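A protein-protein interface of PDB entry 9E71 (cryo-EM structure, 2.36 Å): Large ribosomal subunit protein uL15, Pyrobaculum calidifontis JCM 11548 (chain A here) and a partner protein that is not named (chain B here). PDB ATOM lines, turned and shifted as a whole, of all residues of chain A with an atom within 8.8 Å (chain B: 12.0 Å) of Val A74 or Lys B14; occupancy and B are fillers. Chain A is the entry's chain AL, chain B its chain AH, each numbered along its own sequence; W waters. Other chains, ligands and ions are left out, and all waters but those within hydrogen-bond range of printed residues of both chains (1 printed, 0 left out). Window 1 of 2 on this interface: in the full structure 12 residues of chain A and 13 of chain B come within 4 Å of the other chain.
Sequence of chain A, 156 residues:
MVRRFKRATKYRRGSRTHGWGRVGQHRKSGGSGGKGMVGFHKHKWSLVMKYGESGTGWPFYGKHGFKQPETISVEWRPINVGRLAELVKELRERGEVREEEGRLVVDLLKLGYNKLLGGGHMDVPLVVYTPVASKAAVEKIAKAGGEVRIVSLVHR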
ATOM      1  N   GLN A  68     -16.409  24.784 -13.661  1.00  0.00           N
ATOM      2  CA  GLN A  68     -17.453  23.894 -14.143  1.00  0.00           C
ATOM      3  C   GLN A  68     -17.187  22.487 -13.621  1.00  0.00           C
ATOM      4  O   GLN A  68     -16.033  22.049 -13.615  1.00  0.00           O
ATOM      5  CB  GLN A  68     -17.505  23.900 -15.665  1.00  0.00           C
ATOM      6  CG  GLN A  68     -18.702  23.191 -16.265  1.00  0.00           C
ATOM      7  CD  GLN A  68     -19.995  23.955 -16.086  1.00  0.00           C
ATOM      8  OE1 GLN A  68     -20.090  24.854 -15.259  1.00  0.00           O
ATOM      9  NE2 GLN A  68     -20.998  23.606 -16.877  1.00  0.00           N
ATOM     10  N   PRO A  69     -18.210  21.766 -13.163  1.00  0.00           N
ATOM     11  CA  PRO A  69     -17.974  20.457 -12.539  1.00  0.00           C
ATOM     12  C   PRO A  69     -17.421  19.438 -13.526  1.00  0.00           C
ATOM     13  O   PRO A  69     -17.958  19.241 -14.620  1.00  0.00           O
ATOM     14  CB  PRO A  69     -19.360  20.056 -12.022  1.00  0.00           C
ATOM     15  CG  PRO A  69     -20.144  21.318 -11.974  1.00  0.00           C
ATOM     16  CD  PRO A  69     -19.610  22.198 -13.042  1.00  0.00           C
ATOM     17  N   GLU A  70     -16.326  18.790 -13.121  1.00  0.00           N
ATOM     18  CA  GLU A  70     -15.644  17.846 -13.997  1.00  0.00           C
ATOM     19  C   GLU A  70     -16.492  16.613 -14.262  1.00  0.00           C
ATOM     20  O   GLU A  70     -16.373  15.999 -15.327  1.00  0.00           O
ATOM     21  CB  GLU A  70     -14.301  17.448 -13.384  1.00  0.00           C
ATOM     22  CG  GLU A  70     -14.268  17.560 -11.866  1.00  0.00           C
ATOM     23  CD  GLU A  70     -12.889  17.325 -11.280  1.00  0.00           C
ATOM     24  OE1 GLU A  70     -11.893  17.675 -11.942  1.00  0.00           O
ATOM     25  OE2 GLU A  70     -12.802  16.791 -10.154  1.00  0.00           O
ATOM     26  N   THR A  71     -17.355  16.239 -13.319  1.00  0.00           N
ATOM     27  CA  THR A  71     -18.205  15.070 -13.509  1.00  0.00           C
ATOM     28  C   THR A  71     -19.315  15.302 -14.520  1.00  0.00           C
ATOM     29  O   THR A  71     -19.931  14.331 -14.968  1.00  0.00           O
ATOM     30  CB  THR A  71     -18.812  14.636 -12.176  1.00  0.00           C
ATOM     31  OG1 THR A  71     -19.308  15.786 -11.481  1.00  0.00           O
ATOM     32  CG2 THR A  71     -17.767  13.938 -11.322  1.00  0.00           C
ATOM     33  N   ILE A  72     -19.596  16.552 -14.882  1.00  0.00           N
ATOM     34  CA  ILE A  72     -20.567  16.870 -15.919  1.00  0.00           C
ATOM     35  C   ILE A  72     -19.916  17.436 -17.166  1.00  0.00           C
ATOM     36  O   ILE A  72     -20.579  17.543 -18.199  1.00  0.00           O
ATOM     37  CB  ILE A  72     -21.652  17.833 -15.400  1.00  0.00           C
ATOM     38  CG1 ILE A  72     -21.046  19.200 -15.079  1.00  0.00           C
ATOM     39  CG2 ILE A  72     -22.341  17.248 -14.186  1.00  0.00           C
ATOM     40  CD1 ILE A  72     -22.064  20.298 -14.948  1.00  0.00           C
ATOM     41  N   SER A  73     -18.642  17.801 -17.103  1.00  0.00           N
ATOM     42  CA  SER A  73     -17.908  18.283 -18.261  1.00  0.00           C
ATOM     43  C   SER A  73     -17.267  17.127 -19.019  1.00  0.00           C
ATOM     44  O   SER A  73     -17.074  16.035 -18.479  1.00  0.00           O
ATOM     45  CB  SER A  73     -16.832  19.282 -17.840  1.00  0.00           C
ATOM     46  OG  SER A  73     -17.327  20.155 -16.844  1.00  0.00           O
ATOM     47  N   VAL A  74     -16.932  17.383 -20.277  1.00  0.00           N
ATOM     48  CA  VAL A  74     -16.287  16.385 -21.122  1.00  0.00           C
ATOM     49  C   VAL A  74     -14.780  16.582 -21.078  1.00  0.00           C
ATOM     50  O   VAL A  74     -14.283  17.714 -21.093  1.00  0.00           O
ATOM     51  CB  VAL A  74     -16.815  16.480 -22.563  1.00  0.00           C
ATOM     52  CG1 VAL A  74     -16.079  15.508 -23.459  1.00  0.00           C
ATOM     53  CG2 VAL A  74     -18.306  16.222 -22.599  1.00  0.00           C
ATOM     54  N   GLU A  75     -14.043  15.475 -21.017  1.00  0.00           N
ATOM     55  CA  GLU A  75     -12.587  15.493 -21.083  1.00  0.00           C
ATOM     56  C   GLU A  75     -12.181  15.213 -22.526  1.00  0.00           C
ATOM     57  O   GLU A  75     -12.298  14.080 -23.003  1.00  0.00           O
ATOM     58  CB  GLU A  75     -11.982  14.474 -20.122  1.00  0.00           C
ATOM     59  CG  GLU A  75     -10.585  14.826 -19.644  1.00  0.00           C
ATOM     60  CD  GLU A  75      -9.780  13.608 -19.226  1.00  0.00           C
ATOM     61  OE1 GLU A  75     -10.198  12.914 -18.275  1.00  0.00           O
ATOM     62  OE2 GLU A  75      -8.729  13.345 -19.844  1.00  0.00           O
ATOM     63  N   TRP A  76     -11.708  16.246 -23.215  1.00  0.00           N
ATOM     64  CA  TRP A  76     -11.443  16.162 -24.642  1.00  0.00           C
ATOM     65  C   TRP A  76     -10.055  15.606 -24.920  1.00  0.00           C
ATOM     66  O   TRP A  76      -9.088  15.920 -24.223  1.00  0.00           O
ATOM     67  CB  TRP A  76     -11.585  17.539 -25.282  1.00  0.00           C
ATOM     68  CG  TRP A  76     -12.964  18.073 -25.199  1.00  0.00           C
ATOM     69  CD1 TRP A  76     -13.431  18.995 -24.315  1.00  0.00           C
ATOM     70  CD2 TRP A  76     -14.066  17.724 -26.035  1.00  0.00           C
ATOM     71  NE1 TRP A  76     -14.760  19.240 -24.544  1.00  0.00           N
ATOM     72  CE2 TRP A  76     -15.173  18.474 -25.600  1.00  0.00           C
ATOM     73  CE3 TRP A  76     -14.224  16.852 -27.111  1.00  0.00           C
ATOM     74  CZ2 TRP A  76     -16.419  18.376 -26.200  1.00  0.00           C
ATOM     75  CZ3 TRP A  76     -15.462  16.756 -27.706  1.00  0.00           C
ATOM     76  CH2 TRP A  76     -16.545  17.514 -27.250  1.00  0.00           C
ATOM     77  N   ARG A  77      -9.965  14.776 -25.955  1.00  0.00           N
ATOM     78  CA  ARG A  77      -8.700  14.232 -26.442  1.00  0.00           C
ATOM     79  C   ARG A  77      -8.655  14.490 -27.938  1.00  0.00           C
ATOM     80  O   ARG A  77      -8.933  13.594 -28.746  1.00  0.00           O
ATOM     81  CB  ARG A  77      -8.572  12.743 -26.132  1.00  0.00           C
ATOM     82  CG  ARG A  77      -9.265  12.320 -24.859  1.00  0.00           C
ATOM     83  CD  ARG A  77      -9.673  10.865 -24.937  1.00  0.00           C
ATOM     84  NE  ARG A  77      -8.569   9.977 -24.596  1.00  0.00           N
ATOM     85  CZ  ARG A  77      -8.643   9.000 -23.703  1.00  0.00           C
ATOM     86  NH1 ARG A  77      -9.770   8.730 -23.067  1.00  0.00           N
ATOM     87  NH2 ARG A  77      -7.559   8.278 -23.443  1.00  0.00           N
ATOM     88  N   ASN A 114     -11.683  12.136 -29.221  1.00  0.00           N
ATOM     89  CA  ASN A 114     -13.060  12.608 -29.265  1.00  0.00           C
ATOM     90  C   ASN A 114     -13.223  13.920 -30.014  1.00  0.00           C
ATOM     91  O   ASN A 114     -14.331  14.464 -30.039  1.00  0.00           O
ATOM     92  CB  ASN A 114     -13.625  12.749 -27.850  1.00  0.00           C
ATOM     93  CG  ASN A 114     -12.621  13.308 -26.877  1.00  0.00           C
ATOM     94  OD1 ASN A 114     -11.730  14.064 -27.255  1.00  0.00           O
ATOM     95  ND2 ASN A 114     -12.766  12.950 -25.611  1.00  0.00           N
ATOM     96  N   LYS A 115     -12.166  14.445 -30.626  1.00  0.00           N
ATOM     97  CA  LYS A 115     -12.282  15.709 -31.338  1.00  0.00           C
ATOM     98  C   LYS A 115     -11.185  15.800 -32.385  1.00  0.00           C
ATOM     99  O   LYS A 115     -10.062  15.348 -32.156  1.00  0.00           O
ATOM    100  CB  LYS A 115     -12.202  16.897 -30.375  1.00  0.00           C
ATOM    101  CG  LYS A 115     -12.547  18.229 -31.006  1.00  0.00           C
ATOM    102  CD  LYS A 115     -11.938  19.371 -30.229  1.00  0.00           C
ATOM    103  CE  LYS A 115     -12.949  20.480 -29.984  1.00  0.00           C
ATOM    104  NZ  LYS A 115     -12.867  21.008 -28.595  1.00  0.00           N
ATOM    105  N   PRO A 131     -17.185  12.859 -32.971  1.00  0.00           N
ATOM    106  CA  PRO A 131     -18.290  13.628 -32.380  1.00  0.00           C
ATOM    107  C   PRO A 131     -18.145  15.125 -32.573  1.00  0.00           C
ATOM    108  O   PRO A 131     -19.155  15.830 -32.679  1.00  0.00           O
ATOM    109  CB  PRO A 131     -18.240  13.233 -30.897  1.00  0.00           C
ATOM    110  CG  PRO A 131     -16.864  12.737 -30.669  1.00  0.00           C
ATOM    111  CD  PRO A 131     -16.366  12.174 -31.959  1.00  0.00           C
ATOM    112  N   VAL A 132     -16.919  15.633 -32.623  1.00  0.00           N
ATOM    113  CA  VAL A 132     -16.665  17.054 -32.814  1.00  0.00           C
ATOM    114  C   VAL A 132     -15.494  17.210 -33.772  1.00  0.00           C
ATOM    115  O   VAL A 132     -14.497  16.488 -33.674  1.00  0.00           O
ATOM    116  CB  VAL A 132     -16.382  17.765 -31.474  1.00  0.00           C
ATOM    117  CG1 VAL A 132     -15.696  19.088 -31.708  1.00  0.00           C
ATOM    118  CG2 VAL A 132     -17.666  17.971 -30.701  1.00  0.00           C
ATOM    119  N   LEU A 153     -23.195  11.376 -29.262  1.00  0.00           N
ATOM    120  CA  LEU A 153     -22.891  10.740 -27.987  1.00  0.00           C
ATOM    121  C   LEU A 153     -24.165  10.625 -27.163  1.00  0.00           C
ATOM    122  O   LEU A 153     -25.087  11.426 -27.320  1.00  0.00           O
ATOM    123  CB  LEU A 153     -21.834  11.532 -27.219  1.00  0.00           C
ATOM    124  CG  LEU A 153     -20.473  11.703 -27.891  1.00  0.00           C
ATOM    125  CD1 LEU A 153     -19.724  12.872 -27.271  1.00  0.00           C
ATOM    126  CD2 LEU A 153     -19.654  10.434 -27.790  1.00  0.00           C
ATOM    127  N   VAL B   9     -17.462  -1.326 -19.381  1.00  0.00           N
ATOM    128  CA  VAL B   9     -17.225  -0.281 -18.386  1.00  0.00           C
ATOM    129  C   VAL B   9     -18.248   0.824 -18.600  1.00  0.00           C
ATOM    130  O   VAL B   9     -18.569   1.146 -19.760  1.00  0.00           O
ATOM    131  CB  VAL B   9     -15.794   0.262 -18.507  1.00  0.00           C
ATOM    132  CG1 VAL B   9     -15.585   1.422 -17.561  1.00  0.00           C
ATOM    133  CG2 VAL B   9     -14.794  -0.838 -18.236  1.00  0.00           C
ATOM    134  N   PRO B  10     -18.817   1.403 -17.543  1.00  0.00           N
ATOM    135  CA  PRO B  10     -19.848   2.432 -17.732  1.00  0.00           C
ATOM    136  C   PRO B  10     -19.277   3.676 -18.392  1.00  0.00           C
ATOM    137  O   PRO B  10     -18.238   4.196 -17.987  1.00  0.00           O
ATOM    138  CB  PRO B  10     -20.337   2.723 -16.310  1.00  0.00           C
ATOM    139  CG  PRO B  10     -19.775   1.662 -15.444  1.00  0.00           C
ATOM    140  CD  PRO B  10     -18.617   1.044 -16.131  1.00  0.00           C
ATOM    141  N   ARG B  11     -19.969   4.147 -19.424  1.00  0.00           N
ATOM    142  CA  ARG B  11     -19.507   5.275 -20.223  1.00  0.00           C
ATOM    143  C   ARG B  11     -19.905   6.569 -19.529  1.00  0.00           C
ATOM    144  O   ARG B  11     -21.067   6.981 -19.583  1.00  0.00           O
ATOM    145  CB  ARG B  11     -20.081   5.215 -21.633  1.00  0.00           C
ATOM    146  CG  ARG B  11     -19.541   6.295 -22.546  1.00  0.00           C
ATOM    147  CD  ARG B  11     -20.204   6.251 -23.904  1.00  0.00           C
ATOM    148  NE  ARG B  11     -21.566   6.761 -23.853  1.00  0.00           N
ATOM    149  CZ  ARG B  11     -22.432   6.676 -24.852  1.00  0.00           C
ATOM    150  NH1 ARG B  11     -22.096   6.143 -26.013  1.00  0.00           N
ATOM    151  NH2 ARG B  11     -23.663   7.147 -24.685  1.00  0.00           N
ATOM    152  N   SER B  12     -18.941   7.210 -18.887  1.00  0.00           N
ATOM    153  CA  SER B  12     -19.185   8.432 -18.147  1.00  0.00           C
ATOM    154  C   SER B  12     -19.221   9.634 -19.086  1.00  0.00           C
ATOM    155  O   SER B  12     -18.737   9.584 -20.218  1.00  0.00           O
ATOM    156  CB  SER B  12     -18.110   8.619 -17.083  1.00  0.00           C
ATOM    157  OG  SER B  12     -16.820   8.509 -17.652  1.00  0.00           O
ATOM    158  N   ILE B  13     -19.813  10.726 -18.597  1.00  0.00           N
ATOM    159  CA  ILE B  13     -19.838  11.962 -19.371  1.00  0.00           C
ATOM    160  C   ILE B  13     -18.436  12.521 -19.538  1.00  0.00           C
ATOM    161  O   ILE B  13     -18.135  13.182 -20.539  1.00  0.00           O
ATOM    162  CB  ILE B  13     -20.774  12.994 -18.715  1.00  0.00           C
ATOM    163  CG1 ILE B  13     -22.194  12.451 -18.617  1.00  0.00           C
ATOM    164  CG2 ILE B  13     -20.765  14.288 -19.497  1.00  0.00           C
ATOM    165  CD1 ILE B  13     -23.090  13.291 -17.746  1.00  0.00           C
ATOM    166  N   LYS B  14     -17.564  12.283 -18.559  1.00  0.00           N
ATOM    167  CA  LYS B  14     -16.186  12.750 -18.651  1.00  0.00           C
ATOM    168  C   LYS B  14     -15.446  12.073 -19.796  1.00  0.00           C
ATOM    169  O   LYS B  14     -14.579  12.683 -20.431  1.00  0.00           O
ATOM    170  CB  LYS B  14     -15.471  12.494 -17.325  1.00  0.00           C
ATOM    171  CG  LYS B  14     -14.154  13.211 -17.169  1.00  0.00           C
ATOM    172  CD  LYS B  14     -13.596  13.023 -15.770  1.00  0.00           C
ATOM    173  CE  LYS B  14     -13.299  11.563 -15.487  1.00  0.00           C
ATOM    174  NZ  LYS B  14     -12.793  11.355 -14.101  1.00  0.00           N
ATOM    175  N   SER B  15     -15.782  10.812 -20.077  1.00  0.00           N
ATOM    176  CA  SER B  15     -15.048  10.042 -21.075  1.00  0.00           C
ATOM    177  C   SER B  15     -15.262  10.579 -22.483  1.00  0.00           C
ATOM    178  O   SER B  15     -14.351  10.505 -23.314  1.00  0.00           O
ATOM    179  CB  SER B  15     -15.455   8.571 -20.998  1.00  0.00           C
ATOM    180  OG  SER B  15     -16.519   8.283 -21.887  1.00  0.00           O
ATOM    181  N   GLY B  16     -16.444  11.113 -22.773  1.00  0.00           N
ATOM    182  CA  GLY B  16     -16.702  11.694 -24.075  1.00  0.00           C
ATOM    183  C   GLY B  16     -17.025  10.709 -25.174  1.00  0.00           C
ATOM    184  O   GLY B  16     -17.016  11.085 -26.348  1.00  0.00           O
ATOM    185  N   GLY B  17     -17.318   9.458 -24.834  1.00  0.00           N
ATOM    186  CA  GLY B  17     -17.654   8.456 -25.820  1.00  0.00           C
ATOM    187  C   GLY B  17     -16.609   7.390 -26.053  1.00  0.00           C
ATOM    188  O   GLY B  17     -16.709   6.661 -27.043  1.00  0.00           O
ATOM    189  N   VAL B  18     -15.601   7.288 -25.197  1.00  0.00           N
ATOM    190  CA  VAL B  18     -14.610   6.224 -25.288  1.00  0.00           C
ATOM    191  C   VAL B  18     -15.048   5.100 -24.358  1.00  0.00           C
ATOM    192  O   VAL B  18     -15.198   5.308 -23.151  1.00  0.00           O
ATOM    193  CB  VAL B  18     -13.210   6.735 -24.919  1.00  0.00           C
ATOM    194  CG1 VAL B  18     -12.150   5.772 -25.415  1.00  0.00           C
ATOM    195  CG2 VAL B  18     -12.985   8.122 -25.490  1.00  0.00           C
ATOM    196  N   THR B  19     -15.255   3.912 -24.915  1.00  0.00           N
ATOM    197  CA  THR B  19     -15.795   2.792 -24.162  1.00  0.00           C
ATOM    198  C   THR B  19     -14.825   1.623 -24.192  1.00  0.00           C
ATOM    199  O   THR B  19     -14.092   1.427 -25.164  1.00  0.00           O
ATOM    200  CB  THR B  19     -17.152   2.346 -24.710  1.00  0.00           C
ATOM    201  OG1 THR B  19     -17.020   2.006 -26.094  1.00  0.00           O
ATOM    202  CG2 THR B  19     -18.171   3.467 -24.562  1.00  0.00           C
ATOM    203  N   LYS B  20     -14.833   0.844 -23.116  1.00  0.00           N
ATOM    204  CA  LYS B  20     -13.916  -0.274 -22.979  1.00  0.00           C
ATOM    205  C   LYS B  20     -14.617  -1.408 -22.248  1.00  0.00           C
ATOM    206  O   LYS B  20     -15.720  -1.253 -21.719  1.00  0.00           O
ATOM    207  CB  LYS B  20     -12.638   0.146 -22.254  1.00  0.00           C
ATOM    208  CG  LYS B  20     -12.868   1.169 -21.170  1.00  0.00           C
ATOM    209  CD  LYS B  20     -11.612   1.397 -20.353  1.00  0.00           C
ATOM    210  CE  LYS B  20     -11.060   0.097 -19.808  1.00  0.00           C
ATOM    211  NZ  LYS B  20     -10.141   0.338 -18.662  1.00  0.00           N
HETATM  212  O   HOH W   1     -18.906  11.524 -15.836  1.00  0.00           O
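N of Glu A75 is in hydrogen-bond range of O of Lys B14 (2.9 Å).
N of Gly B17 sits at hydrogen-bond distance from OG of Ser B15.
O of Arg A77 sits at hydrogen-bond distance from N of Asn A114.
The side-chain hydroxyl (OG) of Ser B15 is in hydrogen-bond range of the backbone carbonyl oxygen (O) of Val B18, at 3.5 Å.
O of Ser B12 lies within hydrogen-bond range of OG of Ser B15, 3.1 Å away.
The side-chain hydroxyl (OG) of Ser A73 is in hydrogen-bond range of the backbone carbonyl oxygen (O) of Pro A69.
The side-chain amide nitrogen (ND2) of Asn A114 sits at hydrogen-bond distance from the backbone carbonyl oxygen (O) of Glu A75.
Ile B13 touches Ile A72 (CG2 to O, 3.5 Å).
Ser A73 touches Ile B13.
O of Ser A73 touches CA of Lys B14, 3.4 Å away.
CG2 of Val A74 touches O of Ile B13, 3.7 Å away.
Val A74 touches Lys B14.
CA of Gly B16 touches CG1 of Val A74 (3.9 Å).
ND2 of Asn A114 touches O of Ser B15, at 3.7 Å.
CD2 of Leu A153 touches O of Gly B16, 3.1 Å away.
Leu A153 touches Gly B17.
Pro A69 touches none of the printed residues of chain B.
No residue of chain B comes within 4 Å of Thr A71.
Of the printed residues of chain B, Ile A72 touches Ile B13 (3.5 Å).
Of the printed residues of chain B, Ser A73 touches Ile B13 (3.7 Å) and Lys B14 (3.4 Å).
No residue of chain B comes within 4 Å of Trp A76.
Printed residues of chain B within 4 Å of Asn A114: Ser B15.
Of the printed residues of chain B, Leu A153 touches Gly B16 (3.1 Å) and Gly B17 (3.4 Å).
Printed residues of chain A within 4 Å of Ile B13: Ile A72 (3.5 Å), Ser A73 (3.7 Å) and Val A74 (3.7 Å).
Printed residues of chain A within 4 Å of Lys B14: Ser A73, Val A74 and Glu A75.
Ser B15 touches just one residue of chain A: Asn A114 (3.7 Å).
Of the printed residues of chain A, Gly B16 touches Val A74 (3.9 Å) and Leu A153 (3.1 Å).
Val B18 touches none of the printed residues of chain A.
The nearest residue of chain B that does not touch Val A74 is Ser B15 (5.1 Å).
The nearest printed residue of chain A that does not touch Lys B14 is Glu A70 (4.01 Å).
The nearest printed residue of chain B that does not touch Asn A114 is Gly B16 (4.1 Å).
Hydrophobic or aromatic side chains of chain B that line the printed part of chain A: Ile B13.
Hydrophobic or aromatic side chains of chain A that line the printed part of chain B: Val A74 and Leu A153.
Water W1 lies within hydrogen-bond range of the backbone NH (N) of Ile B13, the backbone carbonyl oxygen (O) of Thr A71 and the backbone NH (N) of Lys B14.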
